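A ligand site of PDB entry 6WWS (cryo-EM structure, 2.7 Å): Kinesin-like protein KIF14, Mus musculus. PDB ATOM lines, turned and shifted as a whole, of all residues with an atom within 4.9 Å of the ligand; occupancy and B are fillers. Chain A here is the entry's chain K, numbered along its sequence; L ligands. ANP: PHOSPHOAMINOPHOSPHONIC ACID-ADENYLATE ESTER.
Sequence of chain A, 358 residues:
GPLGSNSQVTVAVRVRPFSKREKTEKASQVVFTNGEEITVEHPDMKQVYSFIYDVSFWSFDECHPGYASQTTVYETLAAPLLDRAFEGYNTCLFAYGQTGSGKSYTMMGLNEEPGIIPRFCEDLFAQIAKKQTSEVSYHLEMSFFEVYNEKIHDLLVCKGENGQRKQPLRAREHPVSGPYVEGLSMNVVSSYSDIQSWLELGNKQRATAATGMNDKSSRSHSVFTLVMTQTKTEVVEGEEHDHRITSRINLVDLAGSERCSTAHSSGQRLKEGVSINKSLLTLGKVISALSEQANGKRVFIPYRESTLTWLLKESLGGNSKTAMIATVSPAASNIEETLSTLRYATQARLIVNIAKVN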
ATOM      1  N   ARG A  14      10.401  -3.437   6.225  1.00  0.00           N
ATOM      2  CA  ARG A  14      11.074  -4.727   6.276  1.00  0.00           C
ATOM      3  C   ARG A  14      11.061  -5.257   7.700  1.00  0.00           C
ATOM      4  O   ARG A  14      11.285  -4.491   8.649  1.00  0.00           O
ATOM      5  CB  ARG A  14      12.511  -4.625   5.780  1.00  0.00           C
ATOM      6  CG  ARG A  14      13.134  -5.954   5.446  1.00  0.00           C
ATOM      7  CD  ARG A  14      14.586  -5.829   5.084  1.00  0.00           C
ATOM      8  NE  ARG A  14      15.117  -7.103   4.604  1.00  0.00           N
ATOM      9  CZ  ARG A  14      16.400  -7.344   4.356  1.00  0.00           C
ATOM     10  NH1 ARG A  14      17.321  -6.406   4.532  1.00  0.00           N
ATOM     11  NH2 ARG A  14      16.761  -8.545   3.919  1.00  0.00           N
ATOM     12  N   ARG A  16      12.845  -8.139  10.161  1.00  0.00           N
ATOM     13  CA  ARG A  16      14.030  -8.977  10.246  1.00  0.00           C
ATOM     14  C   ARG A  16      13.654 -10.356  10.780  1.00  0.00           C
ATOM     15  O   ARG A  16      12.569 -10.508  11.363  1.00  0.00           O
ATOM     16  CB  ARG A  16      15.098  -8.323  11.111  1.00  0.00           C
ATOM     17  CG  ARG A  16      14.911  -8.391  12.621  1.00  0.00           C
ATOM     18  CD  ARG A  16      16.122  -7.831  13.319  1.00  0.00           C
ATOM     19  NE  ARG A  16      15.823  -7.398  14.685  1.00  0.00           N
ATOM     20  CZ  ARG A  16      15.575  -8.214  15.703  1.00  0.00           C
ATOM     21  NH1 ARG A  16      15.562  -9.538  15.549  1.00  0.00           N
ATOM     22  NH2 ARG A  16      15.327  -7.706  16.903  1.00  0.00           N
ATOM     23  N   PRO A  17      14.512 -11.366  10.609  1.00  0.00           N
ATOM     24  CA  PRO A  17      14.245 -12.667  11.232  1.00  0.00           C
ATOM     25  C   PRO A  17      14.830 -12.726  12.628  1.00  0.00           C
ATOM     26  O   PRO A  17      15.600 -11.841  13.019  1.00  0.00           O
ATOM     27  CB  PRO A  17      14.943 -13.634  10.277  1.00  0.00           C
ATOM     28  CG  PRO A  17      16.144 -12.880   9.868  1.00  0.00           C
ATOM     29  CD  PRO A  17      15.709 -11.430   9.752  1.00  0.00           C
ATOM     30  N   SER A  59      11.121 -10.682   5.560  1.00  0.00           N
ATOM     31  CA  SER A  59      12.323 -11.462   5.790  1.00  0.00           C
ATOM     32  C   SER A  59      12.263 -12.013   7.216  1.00  0.00           C
ATOM     33  O   SER A  59      12.911 -11.483   8.123  1.00  0.00           O
ATOM     34  CB  SER A  59      13.565 -10.614   5.586  1.00  0.00           C
ATOM     35  OG  SER A  59      13.629  -9.579   6.542  1.00  0.00           O
ATOM     36  N   TYR A  67       9.295 -14.164   0.371  1.00  0.00           N
ATOM     37  CA  TYR A  67      10.555 -13.816   0.999  1.00  0.00           C
ATOM     38  C   TYR A  67      11.240 -12.689   0.231  1.00  0.00           C
ATOM     39  O   TYR A  67      11.100 -12.587  -0.987  1.00  0.00           O
ATOM     40  CB  TYR A  67      11.473 -15.029   1.057  1.00  0.00           C
ATOM     41  CG  TYR A  67      12.726 -14.828   1.881  1.00  0.00           C
ATOM     42  CD1 TYR A  67      12.656 -14.566   3.230  1.00  0.00           C
ATOM     43  CD2 TYR A  67      13.977 -14.903   1.298  1.00  0.00           C
ATOM     44  CE1 TYR A  67      13.790 -14.380   3.985  1.00  0.00           C
ATOM     45  CE2 TYR A  67      15.115 -14.717   2.036  1.00  0.00           C
ATOM     46  CZ  TYR A  67      15.022 -14.455   3.380  1.00  0.00           C
ATOM     47  OH  TYR A  67      16.166 -14.268   4.126  1.00  0.00           O
ATOM     48  N   GLN A  70      18.208  -9.456  -0.176  1.00  0.00           N
ATOM     49  CA  GLN A  70      18.824  -8.190  -0.547  1.00  0.00           C
ATOM     50  C   GLN A  70      18.757  -7.922  -2.046  1.00  0.00           C
ATOM     51  O   GLN A  70      18.821  -6.753  -2.459  1.00  0.00           O
ATOM     52  CB  GLN A  70      20.282  -8.156  -0.095  1.00  0.00           C
ATOM     53  CG  GLN A  70      20.478  -8.276   1.409  1.00  0.00           C
ATOM     54  CD  GLN A  70      19.779  -7.204   2.202  1.00  0.00           C
ATOM     55  OE1 GLN A  70      19.087  -7.488   3.172  1.00  0.00           O
ATOM     56  NE2 GLN A  70      19.936  -5.951   1.785  1.00  0.00           N
ATOM     57  N   GLN A  98      15.246   1.378  14.448  1.00  0.00           N
ATOM     58  CA  GLN A  98      15.773   1.467  15.788  1.00  0.00           C
ATOM     59  C   GLN A  98      16.854   0.410  15.941  1.00  0.00           C
ATOM     60  O   GLN A  98      16.964  -0.504  15.123  1.00  0.00           O
ATOM     61  CB  GLN A  98      14.673   1.292  16.841  1.00  0.00           C
ATOM     62  CG  GLN A  98      14.141   2.607  17.362  1.00  0.00           C
ATOM     63  CD  GLN A  98      15.024   3.202  18.434  1.00  0.00           C
ATOM     64  OE1 GLN A  98      16.210   2.921  18.501  1.00  0.00           O
ATOM     65  NE2 GLN A  98      14.429   4.033  19.283  1.00  0.00           N
ATOM     66  N   THR A  99      17.661   0.559  16.989  1.00  0.00           N
ATOM     67  CA  THR A  99      18.874  -0.230  17.115  1.00  0.00           C
ATOM     68  C   THR A  99      18.558  -1.698  17.314  1.00  0.00           C
ATOM     69  O   THR A  99      18.031  -2.095  18.365  1.00  0.00           O
ATOM     70  CB  THR A  99      19.730   0.308  18.265  1.00  0.00           C
ATOM     71  OG1 THR A  99      19.924   1.713  18.110  1.00  0.00           O
ATOM     72  CG2 THR A  99      21.073  -0.363  18.248  1.00  0.00           C
ATOM     73  N   GLY A 100      18.874  -2.509  16.312  1.00  0.00           N
ATOM     74  CA  GLY A 100      18.524  -3.915  16.271  1.00  0.00           C
ATOM     75  C   GLY A 100      17.484  -4.267  15.231  1.00  0.00           C
ATOM     76  O   GLY A 100      16.989  -5.411  15.226  1.00  0.00           O
ATOM     77  N   SER A 101      17.137  -3.341  14.342  1.00  0.00           N
ATOM     78  CA  SER A 101      16.056  -3.530  13.391  1.00  0.00           C
ATOM     79  C   SER A 101      16.499  -4.140  12.072  1.00  0.00           C
ATOM     80  O   SER A 101      15.722  -4.892  11.470  1.00  0.00           O
ATOM     81  CB  SER A 101      15.382  -2.186  13.127  1.00  0.00           C
ATOM     82  OG  SER A 101      16.271  -1.292  12.474  1.00  0.00           O
ATOM     83  N   GLY A 102      17.709  -3.839  11.617  1.00  0.00           N
ATOM     84  CA  GLY A 102      18.172  -4.243  10.306  1.00  0.00           C
ATOM     85  C   GLY A 102      18.492  -3.080   9.395  1.00  0.00           C
ATOM     86  O   GLY A 102      18.466  -3.241   8.171  1.00  0.00           O
ATOM     87  N   LYS A 103      18.808  -1.916   9.964  1.00  0.00           N
ATOM     88  CA  LYS A 103      19.089  -0.730   9.168  1.00  0.00           C
ATOM     89  C   LYS A 103      20.443  -0.835   8.466  1.00  0.00           C
ATOM     90  O   LYS A 103      20.524  -0.678   7.239  1.00  0.00           O
ATOM     91  CB  LYS A 103      19.037   0.496  10.066  1.00  0.00           C
ATOM     92  CG  LYS A 103      19.138   1.839   9.363  1.00  0.00           C
ATOM     93  CD  LYS A 103      19.249   2.973  10.371  1.00  0.00           C
ATOM     94  CE  LYS A 103      17.934   3.247  11.050  1.00  0.00           C
ATOM     95  NZ  LYS A 103      18.020   4.388  11.999  1.00  0.00           N
ATOM     96  N   SER A 104      21.505  -1.080   9.222  1.00  0.00           N
ATOM     97  CA  SER A 104      22.841  -1.190   8.658  1.00  0.00           C
ATOM     98  C   SER A 104      23.047  -2.451   7.837  1.00  0.00           C
ATOM     99  O   SER A 104      23.998  -2.513   7.066  1.00  0.00           O
ATOM    100  CB  SER A 104      23.882  -1.141   9.778  1.00  0.00           C
ATOM    101  OG  SER A 104      23.986   0.172  10.308  1.00  0.00           O
ATOM    102  N   TYR A 105      22.176  -3.443   7.992  1.00  0.00           N
ATOM    103  CA  TYR A 105      22.196  -4.640   7.163  1.00  0.00           C
ATOM    104  C   TYR A 105      21.458  -4.452   5.849  1.00  0.00           C
ATOM    105  O   TYR A 105      21.913  -4.995   4.828  1.00  0.00           O
ATOM    106  CB  TYR A 105      21.570  -5.803   7.945  1.00  0.00           C
ATOM    107  CG  TYR A 105      21.435  -7.104   7.188  1.00  0.00           C
ATOM    108  CD1 TYR A 105      20.293  -7.403   6.468  1.00  0.00           C
ATOM    109  CD2 TYR A 105      22.451  -8.048   7.224  1.00  0.00           C
ATOM    110  CE1 TYR A 105      20.167  -8.591   5.783  1.00  0.00           C
ATOM    111  CE2 TYR A 105      22.337  -9.243   6.542  1.00  0.00           C
ATOM    112  CZ  TYR A 105      21.189  -9.507   5.826  1.00  0.00           C
ATOM    113  OH  TYR A 105      21.065 -10.687   5.154  1.00  0.00           O
ATOM    114  N   ASN A 214      21.715  -0.526  23.272  1.00  0.00           N
ATOM    115  CA  ASN A 214      22.847  -1.111  22.584  1.00  0.00           C
ATOM    116  C   ASN A 214      24.135  -0.468  23.091  1.00  0.00           C
ATOM    117  O   ASN A 214      24.124   0.599  23.698  1.00  0.00           O
ATOM    118  CB  ASN A 214      22.698  -0.942  21.079  1.00  0.00           C
ATOM    119  CG  ASN A 214      23.752  -1.704  20.275  1.00  0.00           C
ATOM    120  OD1 ASN A 214      24.237  -2.749  20.706  1.00  0.00           O
ATOM    121  ND2 ASN A 214      24.134  -1.152  19.124  1.00  0.00           N
ATOM    122  N   LYS A 216      26.419   0.675  21.066  1.00  0.00           N
ATOM    123  CA  LYS A 216      26.762   1.731  20.108  1.00  0.00           C
ATOM    124  C   LYS A 216      25.503   2.139  19.353  1.00  0.00           C
ATOM    125  O   LYS A 216      25.126   1.488  18.379  1.00  0.00           O
ATOM    126  CB  LYS A 216      27.853   1.257  19.161  1.00  0.00           C
ATOM    127  CG  LYS A 216      28.512   2.371  18.363  1.00  0.00           C
ATOM    128  CD  LYS A 216      29.533   1.818  17.371  1.00  0.00           C
ATOM    129  CE  LYS A 216      30.847   1.445  18.049  1.00  0.00           C
ATOM    130  NZ  LYS A 216      31.601   2.620  18.535  1.00  0.00           N
HETATM  131  PG  ANP L   1      21.859   0.428  13.633  1.00  0.00           P
HETATM  132  O1G ANP L   1      20.702   1.373  13.630  1.00  0.00           O
HETATM  133  O2G ANP L   1      22.709   0.644  12.321  1.00  0.00           O
HETATM  134  O3G ANP L   1      22.761   0.720  14.891  1.00  0.00           O
HETATM  135  PB  ANP L   1      22.472  -2.177  14.283  1.00  0.00           P
HETATM  136  O1B ANP L   1      23.803  -1.512  14.201  1.00  0.00           O
HETATM  137  O2B ANP L   1      22.164  -2.529  15.768  1.00  0.00           O
HETATM  138  N3B ANP L   1      21.287  -1.160  13.686  1.00  0.00           N
HETATM  139  PA  ANP L   1      23.370  -4.687  14.031  1.00  0.00           P
HETATM  140  O1A ANP L   1      24.603  -4.864  13.237  1.00  0.00           O
HETATM  141  O2A ANP L   1      23.606  -4.369  15.509  1.00  0.00           O
HETATM  142  O3A ANP L   1      22.498  -3.501  13.462  1.00  0.00           O
HETATM  143  O5' ANP L   1      22.488  -5.972  13.849  1.00  0.00           O
HETATM  144  C5' ANP L   1      21.904  -6.259  12.576  1.00  0.00           C
HETATM  145  C4' ANP L   1      21.800  -7.752  12.409  1.00  0.00           C
HETATM  146  O4' ANP L   1      20.524  -8.063  11.836  1.00  0.00           O
HETATM  147  C3' ANP L   1      22.841  -8.388  11.481  1.00  0.00           C
HETATM  148  O3' ANP L   1      23.913  -8.937  12.243  1.00  0.00           O
HETATM  149  C2' ANP L   1      22.062  -9.489  10.723  1.00  0.00           C
HETATM  150  O2' ANP L   1      22.529 -10.781  11.064  1.00  0.00           O
HETATM  151  C1' ANP L   1      20.610  -9.308  11.176  1.00  0.00           C
HETATM  152  N9  ANP L   1      19.648  -9.280  10.091  1.00  0.00           N
HETATM  153  C8  ANP L   1      18.840  -8.226   9.734  1.00  0.00           C
HETATM  154  N7  ANP L   1      18.064  -8.466   8.712  1.00  0.00           N
HETATM  155  C5  ANP L   1      18.376  -9.773   8.360  1.00  0.00           C
HETATM  156  C6  ANP L   1      17.905 -10.615   7.338  1.00  0.00           C
HETATM  157  N6  ANP L   1      16.963 -10.260   6.460  1.00  0.00           N
HETATM  158  N1  ANP L   1      18.435 -11.856   7.260  1.00  0.00           N
HETATM  159  C2  ANP L   1      19.372 -12.219   8.142  1.00  0.00           C
HETATM  160  N3  ANP L   1      19.903 -11.511   9.138  1.00  0.00           N
HETATM  161  C4  ANP L   1      19.353 -10.285   9.194  1.00  0.00           C
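The side-chain hydroxyl (OG) of Ser 104 is in hydrogen-bond range of an oxygen (O2G) of the ligand (2.4 Å).
The side-chain hydroxyl (OG) of Ser 59 lies within hydrogen-bond range of a nitrogen (N6) of the ligand, at 3.4 Å.
N of Gly 100 sits at hydrogen-bond distance from O2B of the ligand (3.3 Å).
The backbone carbonyl oxygen (O) of Gly 100 lies close to the guanidinium group (NH2) of Arg 16 (3.3 Å).
The guanidinium group (NH1) of Arg 14 lies within hydrogen-bond range of the side-chain amide oxygen (OE1) of Gln 70, at 2.5 Å.
NE of Arg 14 is in hydrogen-bond range of OG of Ser 59 (3.5 Å).
NH2 of Arg 14 sits close to N6 of the ligand.
Merely in contact with the ligand: Arg 16, Pro 17, Thr 99, Lys 103 and Tyr 105.
Hydrophobic or aromatic side chains within 4 Å of the ligand: Pro 17 and Tyr 105.
Nine residues have an atom within 4 Å of the ligand: Arg 14, Arg 16, Pro 17, Ser 59, Thr 99, Gly 100, Lys 103, Ser 104 and Tyr 105.
Along chain A the residues within 4 Å of the ligand span positions 14 to 105.
The nearest printed residue that does not touch the ligand is Gly 102 (4.1 Å).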
